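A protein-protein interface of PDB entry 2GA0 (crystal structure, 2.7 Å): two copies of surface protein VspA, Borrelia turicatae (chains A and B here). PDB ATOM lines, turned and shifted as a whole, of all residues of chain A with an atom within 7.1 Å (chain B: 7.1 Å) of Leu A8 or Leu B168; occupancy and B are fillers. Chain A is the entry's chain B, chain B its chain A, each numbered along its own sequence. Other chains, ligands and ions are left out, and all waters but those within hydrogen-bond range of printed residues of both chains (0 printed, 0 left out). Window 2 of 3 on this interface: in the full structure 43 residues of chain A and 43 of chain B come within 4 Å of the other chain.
Leu A8 touches Leu B168, and with the chains exchanged Leu A168 touches Leu B8.
Thr A12 touches Leu B168, and with the chains exchanged Leu A168 touches Thr B12.
Leu A168 touches its own counterpart, Leu B168.
Of the 7 pairs that touch across the chains among the printed residues, 5 have their exchanged pair printed and touching as well.
Leu A8 touches just one residue of chain B: Leu B168 (3.5 Å).
Printed residues of chain B within 4 Å of Ile A15: Ile B165.
Of the printed residues of chain A, Leu B8 touches Leu A168.
Printed residues of chain A within 4 Å of Thr B12: Leu A168 (3.4 Å).
Printed residues of chain B within 4 Å of Leu A168: Leu B8 (3.7 Å), Thr B12 (3.4 Å) and Leu B168 (3.97 Å).
Leu A8 touches Leu B168.
CG2 of Thr A12 touches CG2 of Ile B165 (3.6 Å).
Leu B168 touches Thr A12.
Ile A15 touches Ile B165 (CG2 to CD1, 3.95 Å).
Leu A168 touches Leu B8 (CD2 to CD1, 3.7 Å).
Thr B12 touches Leu A168 (OG1 to CD1, 3.4 Å).
Leu B168 touches Leu A168.
The side-chain hydroxyl of Thr B12 sits close to the backbone carbonyl oxygen of Leu B8, 3.4 Å away.
The backbone carbonyl oxygen (O) of Leu A8 lies within hydrogen-bond range of the side-chain hydroxyl (OG1) of Thr A12.
Of the 12 printed residues of chain B, 4 touch a printed residue of chain A.
Printed residues of chain B that touch a printed residue of chain A: Leu B8, Thr B12, Ile B165 and Leu B168.
Hydrophobic or aromatic side chains of chain B within 4 Å of the printed part of chain A: Leu B8, Ile B165 and Leu B168.
Of the 11 printed residues of chain A, 4 touch a printed residue of chain B.
Printed residues of chain A that touch a printed residue of chain B: Leu A8, Thr A12, Ile A15 and Leu A168.
Among the printed residues, no Asp or Glu carboxylate lies within 4 Å of a Lys or Arg side-chain nitrogen of the other chain.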
ATOM      1  N   ILE A   6     -21.994 -19.636  22.349  1.00  0.00           N
ATOM      2  CA  ILE A   6     -20.858 -20.531  22.097  1.00  0.00           C
ATOM      3  C   ILE A   6     -20.203 -20.023  20.797  1.00  0.00           C
ATOM      4  O   ILE A   6     -20.596 -18.920  20.374  1.00  0.00           O
ATOM      5  CB  ILE A   6     -21.341 -21.964  21.815  1.00  0.00           C
ATOM      6  CG1 ILE A   6     -22.800 -22.185  22.212  1.00  0.00           C
ATOM      7  CG2 ILE A   6     -20.310 -23.009  22.301  1.00  0.00           C
ATOM      8  CD1 ILE A   6     -23.787 -21.845  21.092  1.00  0.00           C
ATOM      9  N   ASP A   7     -19.275 -20.793  20.158  1.00  0.00           N
ATOM     10  CA  ASP A   7     -18.777 -20.479  18.790  1.00  0.00           C
ATOM     11  C   ASP A   7     -17.863 -21.545  18.030  1.00  0.00           C
ATOM     12  O   ASP A   7     -16.704 -21.794  18.424  1.00  0.00           O
ATOM     13  CB  ASP A   7     -18.100 -19.092  18.808  1.00  0.00           C
ATOM     14  CG  ASP A   7     -17.725 -18.574  17.412  1.00  0.00           C
ATOM     15  OD1 ASP A   7     -17.933 -19.265  16.391  1.00  0.00           O
ATOM     16  OD2 ASP A   7     -17.203 -17.457  17.233  1.00  0.00           O
ATOM     17  N   LEU A   8     -18.344 -22.120  16.910  1.00  0.00           N
ATOM     18  CA  LEU A   8     -17.657 -23.306  16.338  1.00  0.00           C
ATOM     19  C   LEU A   8     -16.964 -23.164  14.998  1.00  0.00           C
ATOM     20  O   LEU A   8     -15.869 -23.685  14.858  1.00  0.00           O
ATOM     21  CB  LEU A   8     -18.514 -24.583  16.379  1.00  0.00           C
ATOM     22  CG  LEU A   8     -18.664 -25.396  17.683  1.00  0.00           C
ATOM     23  CD1 LEU A   8     -19.580 -24.724  18.738  1.00  0.00           C
ATOM     24  CD2 LEU A   8     -19.181 -26.787  17.351  1.00  0.00           C
ATOM     25  N   ALA A   9     -17.573 -22.468  14.038  1.00  0.00           N
ATOM     26  CA  ALA A   9     -17.011 -22.308  12.693  1.00  0.00           C
ATOM     27  C   ALA A   9     -15.652 -21.595  12.677  1.00  0.00           C
ATOM     28  O   ALA A   9     -14.700 -22.054  12.015  1.00  0.00           O
ATOM     29  CB  ALA A   9     -18.005 -21.577  11.788  1.00  0.00           C
ATOM     30  N   THR A  10     -15.586 -20.469  13.395  1.00  0.00           N
ATOM     31  CA  THR A  10     -14.353 -19.687  13.519  1.00  0.00           C
ATOM     32  C   THR A  10     -13.280 -20.470  14.265  1.00  0.00           C
ATOM     33  O   THR A  10     -12.096 -20.457  13.872  1.00  0.00           O
ATOM     34  CB  THR A  10     -14.582 -18.325  14.194  1.00  0.00           C
ATOM     35  OG1 THR A  10     -15.931 -18.229  14.676  1.00  0.00           O
ATOM     36  CG2 THR A  10     -14.492 -17.211  13.155  1.00  0.00           C
ATOM     37  N   ILE A  11     -13.689 -21.170  15.325  1.00  0.00           N
ATOM     38  CA  ILE A  11     -12.740 -21.994  16.084  1.00  0.00           C
ATOM     39  C   ILE A  11     -12.214 -23.173  15.270  1.00  0.00           C
ATOM     40  O   ILE A  11     -11.027 -23.461  15.303  1.00  0.00           O
ATOM     41  CB  ILE A  11     -13.283 -22.421  17.472  1.00  0.00           C
ATOM     42  CG1 ILE A  11     -12.987 -21.314  18.495  1.00  0.00           C
ATOM     43  CG2 ILE A  11     -12.652 -23.759  17.927  1.00  0.00           C
ATOM     44  CD1 ILE A  11     -13.997 -21.165  19.612  1.00  0.00           C
ATOM     45  N   THR A  12     -13.097 -23.823  14.518  1.00  0.00           N
ATOM     46  CA  THR A  12     -12.708 -24.874  13.588  1.00  0.00           C
ATOM     47  C   THR A  12     -11.712 -24.379  12.523  1.00  0.00           C
ATOM     48  O   THR A  12     -10.683 -25.014  12.314  1.00  0.00           O
ATOM     49  CB  THR A  12     -13.976 -25.484  12.961  1.00  0.00           C
ATOM     50  OG1 THR A  12     -14.691 -26.217  13.961  1.00  0.00           O
ATOM     51  CG2 THR A  12     -13.628 -26.538  11.911  1.00  0.00           C
ATOM     52  N   LYS A  13     -12.013 -23.255  11.873  1.00  0.00           N
ATOM     53  CA  LYS A  13     -11.111 -22.685  10.884  1.00  0.00           C
ATOM     54  C   LYS A  13      -9.743 -22.404  11.508  1.00  0.00           C
ATOM     55  O   LYS A  13      -8.721 -22.728  10.920  1.00  0.00           O
ATOM     56  CB  LYS A  13     -11.695 -21.426  10.253  1.00  0.00           C
ATOM     57  CG  LYS A  13     -11.140 -21.141   8.857  1.00  0.00           C
ATOM     58  CD  LYS A  13     -10.497 -19.754   8.743  1.00  0.00           C
ATOM     59  CE  LYS A  13     -11.068 -18.769   9.764  1.00  0.00           C
ATOM     60  NZ  LYS A  13     -10.198 -17.580   9.963  1.00  0.00           N
ATOM     61  N   ASN A  14      -9.738 -21.850  12.719  1.00  0.00           N
ATOM     62  CA  ASN A  14      -8.499 -21.546  13.432  1.00  0.00           C
ATOM     63  C   ASN A  14      -7.623 -22.762  13.740  1.00  0.00           C
ATOM     64  O   ASN A  14      -6.398 -22.680  13.660  1.00  0.00           O
ATOM     65  CB  ASN A  14      -8.783 -20.760  14.716  1.00  0.00           C
ATOM     66  CG  ASN A  14      -9.256 -19.320  14.451  1.00  0.00           C
ATOM     67  OD1 ASN A  14      -9.200 -18.813  13.330  1.00  0.00           O
ATOM     68  ND2 ASN A  14      -9.733 -18.664  15.500  1.00  0.00           N
ATOM     69  N   ILE A  15      -8.236 -23.888  14.090  1.00  0.00           N
ATOM     70  CA  ILE A  15      -7.475 -25.120  14.301  1.00  0.00           C
ATOM     71  C   ILE A  15      -6.950 -25.647  12.972  1.00  0.00           C
ATOM     72  O   ILE A  15      -5.791 -26.033  12.893  1.00  0.00           O
ATOM     73  CB  ILE A  15      -8.309 -26.211  15.064  1.00  0.00           C
ATOM     74  CG1 ILE A  15      -8.749 -25.719  16.449  1.00  0.00           C
ATOM     75  CG2 ILE A  15      -7.555 -27.543  15.183  1.00  0.00           C
ATOM     76  CD1 ILE A  15      -9.731 -26.623  17.094  1.00  0.00           C
ATOM     77  N   LEU A 168     -11.050 -23.777  22.004  1.00  0.00           N
ATOM     78  CA  LEU A 168     -12.285 -24.520  21.751  1.00  0.00           C
ATOM     79  C   LEU A 168     -13.213 -24.303  22.894  1.00  0.00           C
ATOM     80  O   LEU A 168     -14.359 -23.977  22.669  1.00  0.00           O
ATOM     81  CB  LEU A 168     -12.051 -26.026  21.665  1.00  0.00           C
ATOM     82  CG  LEU A 168     -12.757 -26.760  20.519  1.00  0.00           C
ATOM     83  CD1 LEU A 168     -12.216 -28.172  20.356  1.00  0.00           C
ATOM     84  CD2 LEU A 168     -14.234 -26.806  20.721  1.00  0.00           C
ATOM     85  N   ILE B   6     -23.260 -32.447  22.836  1.00  0.00           N
ATOM     86  CA  ILE B   6     -21.963 -32.876  22.336  1.00  0.00           C
ATOM     87  C   ILE B   6     -20.835 -32.711  23.386  1.00  0.00           C
ATOM     88  O   ILE B   6     -20.822 -31.735  24.144  1.00  0.00           O
ATOM     89  CB  ILE B   6     -21.667 -32.159  20.966  1.00  0.00           C
ATOM     90  CG1 ILE B   6     -20.986 -33.127  19.976  1.00  0.00           C
ATOM     91  CG2 ILE B   6     -20.891 -30.841  21.150  1.00  0.00           C
ATOM     92  CD1 ILE B   6     -21.934 -33.725  18.905  1.00  0.00           C
ATOM     93  N   LEU B   8     -17.545 -31.736  24.087  1.00  0.00           N
ATOM     94  CA  LEU B   8     -16.346 -30.935  23.816  1.00  0.00           C
ATOM     95  C   LEU B   8     -15.044 -31.668  24.101  1.00  0.00           C
ATOM     96  O   LEU B   8     -14.117 -31.655  23.279  1.00  0.00           O
ATOM     97  CB  LEU B   8     -16.372 -29.674  24.687  1.00  0.00           C
ATOM     98  CG  LEU B   8     -16.222 -28.253  24.138  1.00  0.00           C
ATOM     99  CD1 LEU B   8     -17.019 -28.031  22.851  1.00  0.00           C
ATOM    100  CD2 LEU B   8     -16.640 -27.228  25.227  1.00  0.00           C
ATOM    101  N   ILE B  11     -14.237 -34.800  21.851  1.00  0.00           N
ATOM    102  CA  ILE B  11     -13.934 -34.236  20.539  1.00  0.00           C
ATOM    103  C   ILE B  11     -12.539 -33.626  20.512  1.00  0.00           C
ATOM    104  O   ILE B  11     -11.793 -33.842  19.555  1.00  0.00           O
ATOM    105  CB  ILE B  11     -15.055 -33.221  20.158  1.00  0.00           C
ATOM    106  CG1 ILE B  11     -16.154 -33.952  19.380  1.00  0.00           C
ATOM    107  CG2 ILE B  11     -14.493 -32.010  19.395  1.00  0.00           C
ATOM    108  CD1 ILE B  11     -17.443 -33.208  19.304  1.00  0.00           C
ATOM    109  N   THR B  12     -12.204 -32.895  21.581  1.00  0.00           N
ATOM    110  CA  THR B  12     -10.883 -32.281  21.799  1.00  0.00           C
ATOM    111  C   THR B  12      -9.751 -33.311  21.849  1.00  0.00           C
ATOM    112  O   THR B  12      -8.703 -33.175  21.158  1.00  0.00           O
ATOM    113  CB  THR B  12     -10.904 -31.498  23.130  1.00  0.00           C
ATOM    114  OG1 THR B  12     -11.135 -30.118  22.865  1.00  0.00           O
ATOM    115  CG2 THR B  12      -9.549 -31.466  23.794  1.00  0.00           C
ATOM    116  N   ILE B  15      -9.068 -34.813  18.402  1.00  0.00           N
ATOM    117  CA  ILE B  15      -8.289 -33.899  17.564  1.00  0.00           C
ATOM    118  C   ILE B  15      -6.822 -34.011  17.954  1.00  0.00           C
ATOM    119  O   ILE B  15      -5.946 -34.200  17.097  1.00  0.00           O
ATOM    120  CB  ILE B  15      -8.796 -32.429  17.753  1.00  0.00           C
ATOM    121  CG1 ILE B  15     -10.028 -32.139  16.883  1.00  0.00           C
ATOM    122  CG2 ILE B  15      -7.735 -31.408  17.409  1.00  0.00           C
ATOM    123  CD1 ILE B  15     -11.030 -31.181  17.524  1.00  0.00           C
ATOM    124  N   THR B 162      -8.682 -34.403   9.688  1.00  0.00           N
ATOM    125  CA  THR B 162      -9.814 -33.660   9.145  1.00  0.00           C
ATOM    126  C   THR B 162     -11.148 -34.188   9.648  1.00  0.00           C
ATOM    127  O   THR B 162     -12.002 -33.378   9.987  1.00  0.00           O
ATOM    128  CB  THR B 162      -9.747 -33.485   7.622  1.00  0.00           C
ATOM    129  OG1 THR B 162      -8.700 -34.313   7.092  1.00  0.00           O
ATOM    130  CG2 THR B 162      -9.221 -32.056   7.282  1.00  0.00           C
ATOM    131  N   ALA B 163     -11.311 -35.510   9.758  1.00  0.00           N
ATOM    132  CA  ALA B 163     -12.530 -36.094  10.354  1.00  0.00           C
ATOM    133  C   ALA B 163     -12.750 -35.623  11.785  1.00  0.00           C
ATOM    134  O   ALA B 163     -13.884 -35.301  12.192  1.00  0.00           O
ATOM    135  CB  ALA B 163     -12.509 -37.596  10.329  1.00  0.00           C
ATOM    136  N   ALA B 164     -11.653 -35.582  12.538  1.00  0.00           N
ATOM    137  CA  ALA B 164     -11.661 -35.180  13.944  1.00  0.00           C
ATOM    138  C   ALA B 164     -11.984 -33.715  14.120  1.00  0.00           C
ATOM    139  O   ALA B 164     -12.626 -33.355  15.076  1.00  0.00           O
ATOM    140  CB  ALA B 164     -10.313 -35.499  14.596  1.00  0.00           C
ATOM    141  N   ILE B 165     -11.526 -32.857  13.222  1.00  0.00           N
ATOM    142  CA  ILE B 165     -11.916 -31.461  13.303  1.00  0.00           C
ATOM    143  C   ILE B 165     -13.358 -31.266  12.799  1.00  0.00           C
ATOM    144  O   ILE B 165     -14.135 -30.507  13.402  1.00  0.00           O
ATOM    145  CB  ILE B 165     -10.941 -30.523  12.598  1.00  0.00           C
ATOM    146  CG1 ILE B 165      -9.487 -30.776  13.053  1.00  0.00           C
ATOM    147  CG2 ILE B 165     -11.331 -29.065  12.885  1.00  0.00           C
ATOM    148  CD1 ILE B 165      -8.384 -30.011  12.209  1.00  0.00           C
ATOM    149  N   ASN B 166     -13.721 -31.973  11.720  1.00  0.00           N
ATOM    150  CA  ASN B 166     -15.065 -31.851  11.130  1.00  0.00           C
ATOM    151  C   ASN B 166     -16.146 -32.417  12.025  1.00  0.00           C
ATOM    152  O   ASN B 166     -17.219 -31.841  12.097  1.00  0.00           O
ATOM    153  CB  ASN B 166     -15.131 -32.508   9.736  1.00  0.00           C
ATOM    154  CG  ASN B 166     -14.425 -31.674   8.641  1.00  0.00           C
ATOM    155  OD1 ASN B 166     -14.129 -30.472   8.823  1.00  0.00           O
ATOM    156  ND2 ASN B 166     -14.158 -32.314   7.490  1.00  0.00           N
ATOM    157  N   ALA B 167     -15.863 -33.549  12.694  1.00  0.00           N
ATOM    158  CA  ALA B 167     -16.807 -34.156  13.649  1.00  0.00           C
ATOM    159  C   ALA B 167     -17.219 -33.120  14.673  1.00  0.00           C
ATOM    160  O   ALA B 167     -18.339 -33.122  15.193  1.00  0.00           O
ATOM    161  CB  ALA B 167     -16.186 -35.320  14.365  1.00  0.00           C
ATOM    162  N   LEU B 168     -16.280 -32.229  14.963  1.00  0.00           N
ATOM    163  CA  LEU B 168     -16.533 -31.132  15.895  1.00  0.00           C
ATOM    164  C   LEU B 168     -17.923 -30.616  15.730  1.00  0.00           C
ATOM    165  O   LEU B 168     -18.593 -30.475  16.735  1.00  0.00           O
ATOM    166  CB  LEU B 168     -15.519 -29.982  15.721  1.00  0.00           C
ATOM    167  CG  LEU B 168     -15.024 -29.191  16.948  1.00  0.00           C
ATOM    168  CD1 LEU B 168     -13.909 -28.188  16.555  1.00  0.00           C
ATOM    169  CD2 LEU B 168     -16.183 -28.495  17.708  1.00  0.00           C
